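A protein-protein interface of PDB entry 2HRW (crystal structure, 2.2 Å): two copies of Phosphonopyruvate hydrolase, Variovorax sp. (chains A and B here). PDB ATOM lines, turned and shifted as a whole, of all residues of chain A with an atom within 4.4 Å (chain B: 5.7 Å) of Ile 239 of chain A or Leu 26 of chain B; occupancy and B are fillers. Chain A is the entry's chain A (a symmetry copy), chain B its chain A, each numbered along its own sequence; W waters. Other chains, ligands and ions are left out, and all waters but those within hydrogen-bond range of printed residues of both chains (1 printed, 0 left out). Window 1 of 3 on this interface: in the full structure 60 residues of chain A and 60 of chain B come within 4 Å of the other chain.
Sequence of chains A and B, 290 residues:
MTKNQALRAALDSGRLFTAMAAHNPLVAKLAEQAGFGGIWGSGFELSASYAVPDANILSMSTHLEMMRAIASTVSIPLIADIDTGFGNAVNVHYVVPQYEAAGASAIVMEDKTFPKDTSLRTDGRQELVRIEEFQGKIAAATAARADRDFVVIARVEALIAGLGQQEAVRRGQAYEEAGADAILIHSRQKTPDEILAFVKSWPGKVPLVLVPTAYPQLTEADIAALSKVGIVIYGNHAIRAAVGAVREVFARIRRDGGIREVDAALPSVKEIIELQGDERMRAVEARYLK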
ATOM      1  N   HIS A  23     -29.224  25.382  -2.078  1.00  0.00           N
ATOM      2  CA  HIS A  23     -29.991  25.624  -3.297  1.00  0.00           C
ATOM      3  C   HIS A  23     -31.508  25.802  -3.059  1.00  0.00           C
ATOM      4  O   HIS A  23     -32.269  26.049  -4.005  1.00  0.00           O
ATOM      5  CB  HIS A  23     -29.747  24.524  -4.337  1.00  0.00           C
ATOM      6  CG  HIS A  23     -29.968  23.152  -3.812  1.00  0.00           C
ATOM      7  ND1 HIS A  23     -29.066  22.526  -2.981  1.00  0.00           N
ATOM      8  CD2 HIS A  23     -31.008  22.297  -3.957  1.00  0.00           C
ATOM      9  CE1 HIS A  23     -29.535  21.344  -2.635  1.00  0.00           C
ATOM     10  NE2 HIS A  23     -30.712  21.180  -3.211  1.00  0.00           N
ATOM     11  N   GLU A  45     -24.943  26.162  -7.500  1.00  0.00           N
ATOM     12  CA  GLU A  45     -25.874  25.221  -6.898  1.00  0.00           C
ATOM     13  C   GLU A  45     -27.290  25.339  -7.403  1.00  0.00           C
ATOM     14  O   GLU A  45     -27.950  24.338  -7.673  1.00  0.00           O
ATOM     15  CB  GLU A  45     -25.894  25.365  -5.376  1.00  0.00           C
ATOM     16  CG  GLU A  45     -24.745  24.676  -4.614  1.00  0.00           C
ATOM     17  CD  GLU A  45     -25.269  23.688  -3.574  1.00  0.00           C
ATOM     18  OE1 GLU A  45     -26.458  23.806  -3.211  1.00  0.00           O
ATOM     19  OE2 GLU A  45     -24.507  22.808  -3.101  1.00  0.00           O
ATOM     20  N   ALA A  48     -27.601  24.332 -10.857  1.00  0.00           N
ATOM     21  CA  ALA A  48     -27.385  22.904 -10.915  1.00  0.00           C
ATOM     22  C   ALA A  48     -28.710  22.211 -10.573  1.00  0.00           C
ATOM     23  O   ALA A  48     -29.109  21.248 -11.235  1.00  0.00           O
ATOM     24  CB  ALA A  48     -26.278  22.512  -9.933  1.00  0.00           C
ATOM     25  N   SER A  49     -29.399  22.726  -9.552  1.00  0.00           N
ATOM     26  CA  SER A  49     -30.674  22.154  -9.092  1.00  0.00           C
ATOM     27  C   SER A  49     -31.761  22.289 -10.181  1.00  0.00           C
ATOM     28  O   SER A  49     -32.835  21.692 -10.109  1.00  0.00           O
ATOM     29  CB  SER A  49     -31.122  22.850  -7.786  1.00  0.00           C
ATOM     30  OG  SER A  49     -31.746  24.107  -8.038  1.00  0.00           O
ATOM     31  N   ASN A 236     -20.316  23.767  -2.938  1.00  0.00           N
ATOM     32  CA  ASN A 236     -21.252  22.938  -3.689  1.00  0.00           C
ATOM     33  C   ASN A 236     -21.522  21.571  -3.080  1.00  0.00           C
ATOM     34  O   ASN A 236     -21.981  20.637  -3.771  1.00  0.00           O
ATOM     35  CB  ASN A 236     -20.671  22.747  -5.077  1.00  0.00           C
ATOM     36  CG  ASN A 236     -19.237  22.263  -5.036  1.00  0.00           C
ATOM     37  OD1 ASN A 236     -18.495  22.490  -5.968  1.00  0.00           O
ATOM     38  ND2 ASN A 236     -18.853  21.590  -3.957  1.00  0.00           N
ATOM     39  N   HIS A 237     -21.271  21.461  -1.781  1.00  0.00           N
ATOM     40  CA  HIS A 237     -21.460  20.205  -1.114  1.00  0.00           C
ATOM     41  C   HIS A 237     -22.931  19.883  -0.878  1.00  0.00           C
ATOM     42  O   HIS A 237     -23.294  18.707  -0.773  1.00  0.00           O
ATOM     43  CB  HIS A 237     -20.622  20.214   0.173  1.00  0.00           C
ATOM     44  CG  HIS A 237     -19.189  20.585  -0.075  1.00  0.00           C
ATOM     45  ND1 HIS A 237     -18.779  21.893  -0.235  1.00  0.00           N
ATOM     46  CD2 HIS A 237     -18.099  19.818  -0.324  1.00  0.00           C
ATOM     47  CE1 HIS A 237     -17.501  21.911  -0.580  1.00  0.00           C
ATOM     48  NE2 HIS A 237     -17.066  20.664  -0.641  1.00  0.00           N
ATOM     49  N   ALA A 238     -23.780  20.907  -0.825  1.00  0.00           N
ATOM     50  CA  ALA A 238     -25.202  20.660  -0.618  1.00  0.00           C
ATOM     51  C   ALA A 238     -25.767  19.892  -1.814  1.00  0.00           C
ATOM     52  O   ALA A 238     -26.318  18.795  -1.681  1.00  0.00           O
ATOM     53  CB  ALA A 238     -25.934  21.953  -0.462  1.00  0.00           C
ATOM     54  N   ILE A 239     -25.615  20.469  -2.995  1.00  0.00           N
ATOM     55  CA  ILE A 239     -26.128  19.816  -4.182  1.00  0.00           C
ATOM     56  C   ILE A 239     -25.427  18.459  -4.432  1.00  0.00           C
ATOM     57  O   ILE A 239     -26.066  17.488  -4.878  1.00  0.00           O
ATOM     58  CB  ILE A 239     -26.022  20.754  -5.419  1.00  0.00           C
ATOM     59  CG1 ILE A 239     -27.047  20.303  -6.463  1.00  0.00           C
ATOM     60  CG2 ILE A 239     -24.567  20.817  -5.957  1.00  0.00           C
ATOM     61  CD1 ILE A 239     -28.488  20.618  -6.076  1.00  0.00           C
ATOM     62  N   ARG A 240     -24.136  18.362  -4.113  1.00  0.00           N
ATOM     63  CA  ARG A 240     -23.456  17.090  -4.326  1.00  0.00           C
ATOM     64  C   ARG A 240     -24.012  16.045  -3.374  1.00  0.00           C
ATOM     65  O   ARG A 240     -24.313  14.943  -3.803  1.00  0.00           O
ATOM     66  CB  ARG A 240     -21.939  17.230  -4.179  1.00  0.00           C
ATOM     67  CG  ARG A 240     -21.280  17.857  -5.400  1.00  0.00           C
ATOM     68  CD  ARG A 240     -19.937  18.462  -5.051  1.00  0.00           C
ATOM     69  NE  ARG A 240     -18.932  17.449  -4.726  1.00  0.00           N
ATOM     70  CZ  ARG A 240     -17.690  17.733  -4.346  1.00  0.00           C
ATOM     71  NH1 ARG A 240     -17.289  19.004  -4.243  1.00  0.00           N
ATOM     72  NH2 ARG A 240     -16.848  16.751  -4.053  1.00  0.00           N
ATOM     73  N   ALA A 241     -24.183  16.398  -2.098  1.00  0.00           N
ATOM     74  CA  ALA A 241     -24.721  15.461  -1.110  1.00  0.00           C
ATOM     75  C   ALA A 241     -26.103  14.954  -1.569  1.00  0.00           C
ATOM     76  O   ALA A 241     -26.395  13.764  -1.521  1.00  0.00           O
ATOM     77  CB  ALA A 241     -24.813  16.141   0.258  1.00  0.00           C
ATOM     78  N   ALA A 242     -26.929  15.875  -2.038  1.00  0.00           N
ATOM     79  CA  ALA A 242     -28.272  15.573  -2.522  1.00  0.00           C
ATOM     80  C   ALA A 242     -28.225  14.643  -3.722  1.00  0.00           C
ATOM     81  O   ALA A 242     -28.890  13.614  -3.741  1.00  0.00           O
ATOM     82  CB  ALA A 242     -28.973  16.861  -2.905  1.00  0.00           C
ATOM     83  N   VAL A 243     -27.450  15.008  -4.738  1.00  0.00           N
ATOM     84  CA  VAL A 243     -27.345  14.164  -5.935  1.00  0.00           C
ATOM     85  C   VAL A 243     -26.905  12.735  -5.558  1.00  0.00           C
ATOM     86  O   VAL A 243     -27.592  11.752  -5.875  1.00  0.00           O
ATOM     87  CB  VAL A 243     -26.359  14.788  -6.996  1.00  0.00           C
ATOM     88  CG1 VAL A 243     -25.886  13.729  -7.996  1.00  0.00           C
ATOM     89  CG2 VAL A 243     -27.061  15.904  -7.759  1.00  0.00           C
ATOM     90  N   ASN B  24     -37.576  19.533  -7.488  1.00  0.00           N
ATOM     91  CA  ASN B  24     -36.842  20.421  -8.396  1.00  0.00           C
ATOM     92  C   ASN B  24     -36.470  19.598  -9.630  1.00  0.00           C
ATOM     93  O   ASN B  24     -36.507  18.372  -9.561  1.00  0.00           O
ATOM     94  CB  ASN B  24     -35.596  21.024  -7.729  1.00  0.00           C
ATOM     95  CG  ASN B  24     -34.632  19.974  -7.198  1.00  0.00           C
ATOM     96  OD1 ASN B  24     -34.403  18.939  -7.830  1.00  0.00           O
ATOM     97  ND2 ASN B  24     -34.037  20.253  -6.034  1.00  0.00           N
ATOM     98  N   PRO B  25     -36.146  20.264 -10.773  1.00  0.00           N
ATOM     99  CA  PRO B  25     -35.771  19.645 -12.049  1.00  0.00           C
ATOM    100  C   PRO B  25     -34.621  18.626 -12.010  1.00  0.00           C
ATOM    101  O   PRO B  25     -34.740  17.566 -12.601  1.00  0.00           O
ATOM    102  CB  PRO B  25     -35.488  20.860 -12.952  1.00  0.00           C
ATOM    103  CG  PRO B  25     -36.479  21.846 -12.477  1.00  0.00           C
ATOM    104  CD  PRO B  25     -36.294  21.724 -10.965  1.00  0.00           C
ATOM    105  N   LEU B  26     -33.521  18.938 -11.329  1.00  0.00           N
ATOM    106  CA  LEU B  26     -32.399  17.994 -11.199  1.00  0.00           C
ATOM    107  C   LEU B  26     -32.906  16.645 -10.613  1.00  0.00           C
ATOM    108  O   LEU B  26     -32.627  15.571 -11.146  1.00  0.00           O
ATOM    109  CB  LEU B  26     -31.316  18.581 -10.258  1.00  0.00           C
ATOM    110  CG  LEU B  26     -30.141  17.684  -9.850  1.00  0.00           C
ATOM    111  CD1 LEU B  26     -29.299  17.394 -11.032  1.00  0.00           C
ATOM    112  CD2 LEU B  26     -29.281  18.341  -8.819  1.00  0.00           C
ATOM    113  N   VAL B  27     -33.645  16.725  -9.508  1.00  0.00           N
ATOM    114  CA  VAL B  27     -34.193  15.547  -8.846  1.00  0.00           C
ATOM    115  C   VAL B  27     -35.107  14.796  -9.795  1.00  0.00           C
ATOM    116  O   VAL B  27     -35.108  13.568  -9.826  1.00  0.00           O
ATOM    117  CB  VAL B  27     -35.007  15.943  -7.573  1.00  0.00           C
ATOM    118  CG1 VAL B  27     -35.903  14.758  -7.109  1.00  0.00           C
ATOM    119  CG2 VAL B  27     -34.053  16.349  -6.458  1.00  0.00           C
ATOM    120  N   ALA B  28     -35.912  15.540 -10.548  1.00  0.00           N
ATOM    121  CA  ALA B  28     -36.821  14.938 -11.531  1.00  0.00           C
ATOM    122  C   ALA B  28     -36.001  14.224 -12.619  1.00  0.00           C
ATOM    123  O   ALA B  28     -36.364  13.131 -13.077  1.00  0.00           O
ATOM    124  CB  ALA B  28     -37.724  16.026 -12.164  1.00  0.00           C
ATOM    125  N   LYS B  29     -34.890  14.844 -13.016  1.00  0.00           N
ATOM    126  CA  LYS B  29     -34.000  14.285 -14.033  1.00  0.00           C
ATOM    127  C   LYS B  29     -33.443  12.971 -13.523  1.00  0.00           C
ATOM    128  O   LYS B  29     -33.444  11.967 -14.229  1.00  0.00           O
ATOM    129  CB  LYS B  29     -32.847  15.240 -14.287  1.00  0.00           C
ATOM    130  CG  LYS B  29     -31.874  14.798 -15.388  1.00  0.00           C
ATOM    131  CD  LYS B  29     -30.929  15.946 -15.703  1.00  0.00           C
ATOM    132  CE  LYS B  29     -30.169  15.741 -16.987  1.00  0.00           C
ATOM    133  NZ  LYS B  29     -29.395  16.972 -17.334  1.00  0.00           N
ATOM    134  N   LEU B  30     -32.951  12.976 -12.291  1.00  0.00           N
ATOM    135  CA  LEU B  30     -32.433  11.747 -11.707  1.00  0.00           C
ATOM    136  C   LEU B  30     -33.479  10.628 -11.661  1.00  0.00           C
ATOM    137  O   LEU B  30     -33.147   9.464 -11.841  1.00  0.00           O
ATOM    138  CB  LEU B  30     -31.906  12.018 -10.307  1.00  0.00           C
ATOM    139  CG  LEU B  30     -30.582  12.804 -10.327  1.00  0.00           C
ATOM    140  CD1 LEU B  30     -30.070  13.073  -8.919  1.00  0.00           C
ATOM    141  CD2 LEU B  30     -29.561  11.974 -11.099  1.00  0.00           C
ATOM    142  N   ALA B  31     -34.731  10.972 -11.415  1.00  0.00           N
ATOM    143  CA  ALA B  31     -35.774   9.959 -11.365  1.00  0.00           C
ATOM    144  C   ALA B  31     -35.947   9.350 -12.737  1.00  0.00           C
ATOM    145  O   ALA B  31     -36.125   8.140 -12.875  1.00  0.00           O
ATOM    146  CB  ALA B  31     -37.094  10.552 -10.889  1.00  0.00           C
ATOM    147  N   THR B  73     -37.393  19.881 -18.468  1.00  0.00           N
ATOM    148  CA  THR B  73     -36.153  19.218 -18.171  1.00  0.00           C
ATOM    149  C   THR B  73     -36.216  17.729 -18.520  1.00  0.00           C
ATOM    150  O   THR B  73     -35.291  17.214 -19.139  1.00  0.00           O
ATOM    151  CB  THR B  73     -35.768  19.426 -16.688  1.00  0.00           C
ATOM    152  OG1 THR B  73     -35.498  20.816 -16.466  1.00  0.00           O
ATOM    153  CG2 THR B  73     -34.527  18.624 -16.326  1.00  0.00           C
ATOM    154  N   ILE B 272     -21.861  16.840 -11.182  1.00  0.00           N
ATOM    155  CA  ILE B 272     -22.951  17.800 -11.111  1.00  0.00           C
ATOM    156  C   ILE B 272     -22.999  18.585 -12.438  1.00  0.00           C
ATOM    157  O   ILE B 272     -24.084  18.814 -12.964  1.00  0.00           O
ATOM    158  CB  ILE B 272     -22.782  18.776  -9.906  1.00  0.00           C
ATOM    159  CG1 ILE B 272     -22.762  17.986  -8.578  1.00  0.00           C
ATOM    160  CG2 ILE B 272     -23.842  19.871  -9.963  1.00  0.00           C
ATOM    161  CD1 ILE B 272     -23.943  17.074  -8.347  1.00  0.00           C
ATOM    162  N   LEU B 275     -24.842  16.636 -15.079  1.00  0.00           N
ATOM    163  CA  LEU B 275     -26.278  16.615 -14.852  1.00  0.00           C
ATOM    164  C   LEU B 275     -26.916  17.959 -15.223  1.00  0.00           C
ATOM    165  O   LEU B 275     -28.106  18.012 -15.505  1.00  0.00           O
ATOM    166  CB  LEU B 275     -26.571  16.289 -13.391  1.00  0.00           C
ATOM    167  CG  LEU B 275     -26.467  14.809 -13.048  1.00  0.00           C
ATOM    168  CD1 LEU B 275     -26.005  14.706 -11.625  1.00  0.00           C
ATOM    169  CD2 LEU B 275     -27.823  14.094 -13.279  1.00  0.00           C
ATOM    170  N   GLN B 276     -26.119  19.032 -15.208  1.00  0.00           N
ATOM    171  CA  GLN B 276     -26.594  20.364 -15.590  1.00  0.00           C
ATOM    172  C   GLN B 276     -26.795  20.496 -17.105  1.00  0.00           C
ATOM    173  O   GLN B 276     -27.389  21.457 -17.587  1.00  0.00           O
ATOM    174  CB  GLN B 276     -25.606  21.430 -15.119  1.00  0.00           C
ATOM    175  CG  GLN B 276     -25.734  21.782 -13.661  1.00  0.00           C
ATOM    176  CD  GLN B 276     -24.731  22.827 -13.240  1.00  0.00           C
ATOM    177  OE1 GLN B 276     -23.524  22.594 -13.253  1.00  0.00           O
ATOM    178  NE2 GLN B 276     -25.224  23.991 -12.868  1.00  0.00           N
HETATM  179  O   HOH W   1     -32.008  18.926  -4.695  1.00  0.00           O
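Water W1 lies within hydrogen-bond range of the side-chain amide nitrogen (ND2) of Asn 24 of chain B (2.8 Å) and a ring nitrogen (NE2) of His 23 of chain A (3.0 Å).
The backbone NH of Leu 26 of chain B is in hydrogen-bond range of the backbone carbonyl oxygen of Ser 49 of chain A (3.1 Å). The backbone NH (N) of Ala 48 of chain A lies close to the side-chain amide nitrogen (NE2) of Gln 276 of chain B, 3.1 Å away.
Among the printed residues, merely in contact across the chains: Ala 48 of chain A with Leu 26 of chain B (3.6 Å), Ala 48 of chain A with Ile 272 of chain B (3.6 Å), Ser 49 of chain A with Asn 24 of chain B (3.7 Å), Ser 49 of chain A with Pro 25 of chain B (3.6 Å), Ile 239 of chain A with Leu 26 of chain B (3.7 Å), Arg 240 of chain A with Ile 272 of chain B (3.5 Å), Val 243 of chain A with Leu 26 of chain B (3.5 Å), Val 243 of chain A with Ile 272 of chain B (3.4 Å) and Val 243 of chain A with Leu 275 of chain B (3.8 Å).
Printed residues of chain A that touch a printed residue of chain B: Ala 48, Ser 49, Ile 239, Arg 240 and Val 243. Printed residues of chain B that touch a printed residue of chain A: Asn 24, Pro 25, Leu 26, Ile 272, Leu 275 and Gln 276. Hydrophobic or aromatic side chains of chain B that line the printed part of chain A: Pro 25, Leu 26, Ile 272 and Leu 275. Among the printed residues, 11 pairs touch across the chains. Among the printed residues, no Asp or Glu carboxylate lies within 4 Å of a Lys or Arg side-chain nitrogen of the other chain.
No position is printed for both chains. Of the 11 pairs that touch across the chains among the printed residues, none has its exchanged pair printed and touching as well.
OD1 of Asn 24 of chain B is in hydrogen-bond range of N of Val 27 of chain B. NZ of Lys 29 of chain B lies within hydrogen-bond range of O of Leu 275 of chain B (2.5 Å). The backbone NH (N) of Ile 239 of chain A is in hydrogen-bond range of the side-chain carboxylate (OE2) of Glu 45 of chain A. The side-chain amide nitrogen of Asn 236 of chain A sits close to the guanidinium group of Arg 240 of chain A, at 3.0 Å.
Printed residues of chain B within 4 Å of Ala 48 of chain A: Leu 26 (3.6 Å), Ile 272 (3.6 Å) and Gln 276 (3.1 Å). Asn 236 of chain A touches none of the printed residues of chain B. Of chain B, only Leu 26 comes within 4 Å of Ile 239 of chain A. Of the printed residues of chain B, Arg 240 of chain A touches Ile 272 (3.5 Å). Printed residues of chain B within 4 Å of Val 243 of chain A: Leu 26, Ile 272 and Leu 275. Of the printed residues of chain A, Pro 25 of chain B touches Ser 49 (3.6 Å). Of chain A, only Ala 48 (3.6 Å), Ser 49 (3.1 Å), Ile 239 (3.7 Å) and Val 243 (3.5 Å) come within 4 Å of Leu 26 of chain B. Ala 28 of chain B touches none of the printed residues of chain A. Of the printed residues of chain A, Ile 272 of chain B touches Ala 48, Arg 240 and Val 243. The nearest residue of chain B that does not touch Ile 239 of chain A is Ile 272 of chain B (4.1 Å). The nearest printed residue of chain A that does not touch Ile 272 of chain B is Ile 239 of chain A (4.1 Å).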
